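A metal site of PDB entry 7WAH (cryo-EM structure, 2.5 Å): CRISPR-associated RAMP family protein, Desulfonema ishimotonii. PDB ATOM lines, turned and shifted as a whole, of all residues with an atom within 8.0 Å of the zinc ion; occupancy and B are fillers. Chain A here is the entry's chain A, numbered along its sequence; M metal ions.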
ATOM      1  N   ARG A 175       0.638  14.393  13.901  1.00  0.00           N
ATOM      2  CA  ARG A 175       0.303  13.416  12.864  1.00  0.00           C
ATOM      3  C   ARG A 175       1.305  13.557  11.719  1.00  0.00           C
ATOM      4  O   ARG A 175       1.378  14.620  11.091  1.00  0.00           O
ATOM      5  CB  ARG A 175      -1.119  13.608  12.367  1.00  0.00           C
ATOM      6  CG  ARG A 175      -1.662  12.425  11.574  1.00  0.00           C
ATOM      7  CD  ARG A 175      -3.174  12.434  11.561  1.00  0.00           C
ATOM      8  NE  ARG A 175      -3.704  11.110  11.245  1.00  0.00           N
ATOM      9  CZ  ARG A 175      -4.221  10.774  10.076  1.00  0.00           C
ATOM     10  NH1 ARG A 175      -4.314  11.636   9.076  1.00  0.00           N
ATOM     11  NH2 ARG A 175      -4.659   9.530   9.901  1.00  0.00           N
ATOM     12  N   ARG A 452       2.516   1.770  13.107  1.00  0.00           N
ATOM     13  CA  ARG A 452       1.783   2.074  11.877  1.00  0.00           C
ATOM     14  C   ARG A 452       2.733   2.399  10.730  1.00  0.00           C
ATOM     15  O   ARG A 452       2.541   1.927   9.603  1.00  0.00           O
ATOM     16  CB  ARG A 452       0.816   3.232  12.137  1.00  0.00           C
ATOM     17  CG  ARG A 452       0.053   3.695  10.910  1.00  0.00           C
ATOM     18  CD  ARG A 452      -0.927   4.806  11.276  1.00  0.00           C
ATOM     19  NE  ARG A 452      -1.894   4.357  12.274  1.00  0.00           N
ATOM     20  CZ  ARG A 452      -3.018   3.724  11.992  1.00  0.00           C
ATOM     21  NH1 ARG A 452      -3.364   3.448  10.745  1.00  0.00           N
ATOM     22  NH2 ARG A 452      -3.830   3.367  12.984  1.00  0.00           N
ATOM     23  N   GLN A 456       3.113   0.202   7.299  1.00  0.00           N
ATOM     24  CA  GLN A 456       2.961   0.823   5.991  1.00  0.00           C
ATOM     25  C   GLN A 456       4.206   0.616   5.130  1.00  0.00           C
ATOM     26  O   GLN A 456       4.104   0.407   3.919  1.00  0.00           O
ATOM     27  CB  GLN A 456       2.657   2.316   6.139  1.00  0.00           C
ATOM     28  CG  GLN A 456       1.303   2.628   6.740  1.00  0.00           C
ATOM     29  CD  GLN A 456       1.125   4.104   7.046  1.00  0.00           C
ATOM     30  OE1 GLN A 456       0.384   4.808   6.363  1.00  0.00           O
ATOM     31  NE2 GLN A 456       1.823   4.579   8.071  1.00  0.00           N
ATOM     32  N   SER A 461       2.517   0.463   0.806  1.00  0.00           N
ATOM     33  CA  SER A 461       1.303   1.179   0.426  1.00  0.00           C
ATOM     34  C   SER A 461       0.929   2.163   1.527  1.00  0.00           C
ATOM     35  O   SER A 461       0.492   1.731   2.612  1.00  0.00           O
ATOM     36  CB  SER A 461       0.158   0.207   0.166  1.00  0.00           C
ATOM     37  OG  SER A 461      -0.136  -0.564   1.319  1.00  0.00           O
ATOM     38  N   PRO A 462       1.095   3.463   1.306  1.00  0.00           N
ATOM     39  CA  PRO A 462       0.697   4.432   2.331  1.00  0.00           C
ATOM     40  C   PRO A 462      -0.803   4.404   2.581  1.00  0.00           C
ATOM     41  O   PRO A 462      -1.604   4.123   1.682  1.00  0.00           O
ATOM     42  CB  PRO A 462       1.135   5.776   1.738  1.00  0.00           C
ATOM     43  CG  PRO A 462       2.173   5.426   0.716  1.00  0.00           C
ATOM     44  CD  PRO A 462       1.745   4.107   0.165  1.00  0.00           C
ATOM     45  N   CYS A 463      -1.188   4.713   3.820  1.00  0.00           N
ATOM     46  CA  CYS A 463      -2.581   4.734   4.229  1.00  0.00           C
ATOM     47  C   CYS A 463      -3.149   6.123   3.974  1.00  0.00           C
ATOM     48  O   CYS A 463      -2.856   7.059   4.720  1.00  0.00           O
ATOM     49  CB  CYS A 463      -2.713   4.340   5.698  1.00  0.00           C
ATOM     50  SG  CYS A 463      -4.375   4.529   6.375  1.00  0.00           S
ATOM     51  N   ASN A 464      -3.969   6.248   2.938  1.00  0.00           N
ATOM     52  CA  ASN A 464      -4.585   7.528   2.586  1.00  0.00           C
ATOM     53  C   ASN A 464      -5.956   7.635   3.252  1.00  0.00           C
ATOM     54  O   ASN A 464      -7.011   7.658   2.609  1.00  0.00           O
ATOM     55  CB  ASN A 464      -4.680   7.676   1.076  1.00  0.00           C
ATOM     56  CG  ASN A 464      -3.324   7.626   0.393  1.00  0.00           C
ATOM     57  OD1 ASN A 464      -2.302   7.918   1.013  1.00  0.00           O
ATOM     58  ND2 ASN A 464      -3.307   7.257  -0.878  1.00  0.00           N
ATOM     59  N   ALA A 465      -5.923   7.678   4.577  1.00  0.00           N
ATOM     60  CA  ALA A 465      -7.129   7.780   5.392  1.00  0.00           C
ATOM     61  C   ALA A 465      -7.177   9.150   6.051  1.00  0.00           C
ATOM     62  O   ALA A 465      -6.208   9.580   6.676  1.00  0.00           O
ATOM     63  CB  ALA A 465      -7.163   6.687   6.454  1.00  0.00           C
ATOM     64  N   GLU A 466      -8.311   9.826   5.917  1.00  0.00           N
ATOM     65  CA  GLU A 466      -8.520  11.117   6.542  1.00  0.00           C
ATOM     66  C   GLU A 466      -9.159  10.944   7.914  1.00  0.00           C
ATOM     67  O   GLU A 466      -9.827   9.945   8.182  1.00  0.00           O
ATOM     68  CB  GLU A 466      -9.394  12.023   5.663  1.00  0.00           C
ATOM     69  CG  GLU A 466      -8.871  12.212   4.236  1.00  0.00           C
ATOM     70  CD  GLU A 466      -7.603  13.047   4.183  1.00  0.00           C
ATOM     71  OE1 GLU A 466      -7.255  13.686   5.193  1.00  0.00           O
ATOM     72  OE2 GLU A 466      -6.964  13.065   3.112  1.00  0.00           O
ATOM     73  N   PRO A 471     -14.255   3.827   9.868  1.00  0.00           N
ATOM     74  CA  PRO A 471     -12.865   3.363   9.953  1.00  0.00           C
ATOM     75  C   PRO A 471     -12.299   2.976   8.599  1.00  0.00           C
ATOM     76  O   PRO A 471     -12.988   2.425   7.742  1.00  0.00           O
ATOM     77  CB  PRO A 471     -12.953   2.152  10.888  1.00  0.00           C
ATOM     78  CG  PRO A 471     -14.206   2.356  11.659  1.00  0.00           C
ATOM     79  CD  PRO A 471     -15.148   3.029  10.723  1.00  0.00           C
ATOM     80  N   CYS A 472     -11.020   3.290   8.408  1.00  0.00           N
ATOM     81  CA  CYS A 472     -10.304   2.882   7.208  1.00  0.00           C
ATOM     82  C   CYS A 472     -10.124   1.365   7.188  1.00  0.00           C
ATOM     83  O   CYS A 472      -9.905   0.728   8.228  1.00  0.00           O
ATOM     84  CB  CYS A 472      -8.948   3.575   7.135  1.00  0.00           C
ATOM     85  SG  CYS A 472      -7.879   3.026   5.784  1.00  0.00           S
ATOM     86  N   MET A 473     -10.219   0.781   5.998  1.00  0.00           N
ATOM     87  CA  MET A 473     -10.180  -0.662   5.825  1.00  0.00           C
ATOM     88  C   MET A 473      -8.910  -1.144   5.113  1.00  0.00           C
ATOM     89  O   MET A 473      -8.913  -2.214   4.512  1.00  0.00           O
ATOM     90  CB  MET A 473     -11.418  -1.146   5.075  1.00  0.00           C
ATOM     91  CG  MET A 473     -12.720  -0.905   5.819  1.00  0.00           C
ATOM     92  SD  MET A 473     -12.735  -1.704   7.436  1.00  0.00           S
ATOM     93  CE  MET A 473     -12.480  -3.414   6.971  1.00  0.00           C
ATOM     94  N   CYS A 474      -7.830  -0.358   5.173  1.00  0.00           N
ATOM     95  CA  CYS A 474      -6.572  -0.798   4.595  1.00  0.00           C
ATOM     96  C   CYS A 474      -5.971  -1.922   5.431  1.00  0.00           C
ATOM     97  O   CYS A 474      -6.446  -2.249   6.517  1.00  0.00           O
ATOM     98  CB  CYS A 474      -5.584   0.362   4.494  1.00  0.00           C
ATOM     99  SG  CYS A 474      -4.806   0.809   6.061  1.00  0.00           S
ATOM    100  N   LYS A 475      -4.908  -2.536   4.898  1.00  0.00           N
ATOM    101  CA  LYS A 475      -4.261  -3.638   5.601  1.00  0.00           C
ATOM    102  C   LYS A 475      -3.642  -3.168   6.912  1.00  0.00           C
ATOM    103  O   LYS A 475      -3.587  -3.924   7.891  1.00  0.00           O
ATOM    104  CB  LYS A 475      -3.204  -4.271   4.696  1.00  0.00           C
ATOM    105  CG  LYS A 475      -3.737  -4.760   3.368  1.00  0.00           C
ATOM    106  CD  LYS A 475      -2.611  -5.283   2.497  1.00  0.00           C
ATOM    107  CE  LYS A 475      -3.112  -5.718   1.130  1.00  0.00           C
ATOM    108  NZ  LYS A 475      -2.000  -6.212   0.277  1.00  0.00           N
ATOM    109  N   THR A 476      -3.146  -1.926   6.945  1.00  0.00           N
ATOM    110  CA  THR A 476      -2.530  -1.397   8.140  1.00  0.00           C
ATOM    111  C   THR A 476      -3.569  -1.097   9.229  1.00  0.00           C
ATOM    112  O   THR A 476      -3.374  -1.471  10.393  1.00  0.00           O
ATOM    113  CB  THR A 476      -1.743  -0.127   7.801  1.00  0.00           C
ATOM    114  OG1 THR A 476      -0.501  -0.480   7.171  1.00  0.00           O
ATOM    115  CG2 THR A 476      -1.476   0.704   9.055  1.00  0.00           C
ATOM    116  N   CYS A 477      -4.674  -0.450   8.858  1.00  0.00           N
ATOM    117  CA  CYS A 477      -5.661  -0.067   9.854  1.00  0.00           C
ATOM    118  C   CYS A 477      -6.380  -1.279  10.450  1.00  0.00           C
ATOM    119  O   CYS A 477      -6.767  -1.251  11.622  1.00  0.00           O
ATOM    120  CB  CYS A 477      -6.678   0.899   9.252  1.00  0.00           C
ATOM    121  SG  CYS A 477      -6.093   2.601   9.136  1.00  0.00           S
ATOM    122  N   ARG A 478      -6.566  -2.327   9.655  1.00  0.00           N
ATOM    123  CA  ARG A 478      -7.144  -3.558  10.189  1.00  0.00           C
ATOM    124  C   ARG A 478      -6.252  -4.152  11.269  1.00  0.00           C
ATOM    125  O   ARG A 478      -6.738  -4.621  12.303  1.00  0.00           O
ATOM    126  CB  ARG A 478      -7.350  -4.573   9.063  1.00  0.00           C
ATOM    127  CG  ARG A 478      -8.407  -4.174   8.054  1.00  0.00           C
ATOM    128  CD  ARG A 478      -8.383  -5.112   6.856  1.00  0.00           C
ATOM    129  NE  ARG A 478      -9.288  -4.682   5.800  1.00  0.00           N
ATOM    130  CZ  ARG A 478      -9.385  -5.262   4.619  1.00  0.00           C
ATOM    131  NH1 ARG A 478      -8.638  -6.299   4.291  1.00  0.00           N
ATOM    132  NH2 ARG A 478     -10.249  -4.785   3.730  1.00  0.00           N
ATOM    133  N   MET A 480      -4.045  -2.439  13.064  1.00  0.00           N
ATOM    134  CA  MET A 480      -3.930  -1.490  14.166  1.00  0.00           C
ATOM    135  C   MET A 480      -5.157  -1.442  15.056  1.00  0.00           C
ATOM    136  O   MET A 480      -5.073  -0.926  16.173  1.00  0.00           O
ATOM    137  CB  MET A 480      -3.628  -0.091  13.630  1.00  0.00           C
ATOM    138  CG  MET A 480      -2.252   0.055  13.000  1.00  0.00           C
ATOM    139  SD  MET A 480      -0.904  -0.407  14.100  1.00  0.00           S
ATOM    140  CE  MET A 480      -1.072   0.793  15.408  1.00  0.00           C
ATOM    141  N   ARG A 481      -6.302  -1.975  14.614  1.00  0.00           N
ATOM    142  CA  ARG A 481      -7.515  -1.954  15.419  1.00  0.00           C
ATOM    143  C   ARG A 481      -7.559  -3.072  16.444  1.00  0.00           C
ATOM    144  O   ARG A 481      -8.388  -3.028  17.357  1.00  0.00           O
ATOM    145  CB  ARG A 481      -8.752  -2.028  14.522  1.00  0.00           C
ATOM    146  CG  ARG A 481      -9.345  -0.678  14.213  1.00  0.00           C
ATOM    147  CD  ARG A 481     -10.665  -0.796  13.462  1.00  0.00           C
ATOM    148  NE  ARG A 481     -10.481  -1.285  12.102  1.00  0.00           N
ATOM    149  CZ  ARG A 481     -10.166  -0.516  11.065  1.00  0.00           C
ATOM    150  NH1 ARG A 481      -9.973   0.783  11.207  1.00  0.00           N
ATOM    151  NH2 ARG A 481     -10.044  -1.069   9.865  1.00  0.00           N
HETATM  152 ZN    ZN M   1      -5.814   2.755   6.824  1.00  0.00          ZN
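The guanidinium group (NH2) of Arg 481 lies within hydrogen-bond range of the backbone carbonyl oxygen (O) of Cys 472 (2.4 Å).
The backbone NH of Cys 463 is in hydrogen-bond range of the side-chain amide oxygen of Gln 456 (3.0 Å).
The guanidinium group (NH1) of Arg 452 sits close to the side-chain sulfur (SG) of Cys 477 (3.3 Å).
The backbone NH (N) of Thr 476 lies close to the side-chain sulfur (SG) of Cys 474 (3.3 Å).
Four residues have an atom within 4 Å of the zinc ion: Cys 463, Cys 472, Cys 474 and Cys 477.
Along chain A the residues within 4 Å of the zinc ion span positions 463 to 477.
The nearest printed residue that does not touch the zinc ion is Ala 465 (4.2 Å).
The zinc ion is bound by the side-chain sulfur of Cys 474 (2.3 Å), the side-chain sulfur of Cys 463 (2.3 Å), the side-chain sulfur of Cys 472 (2.3 Å) and the side-chain sulfur of Cys 477 (2.3 Å).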
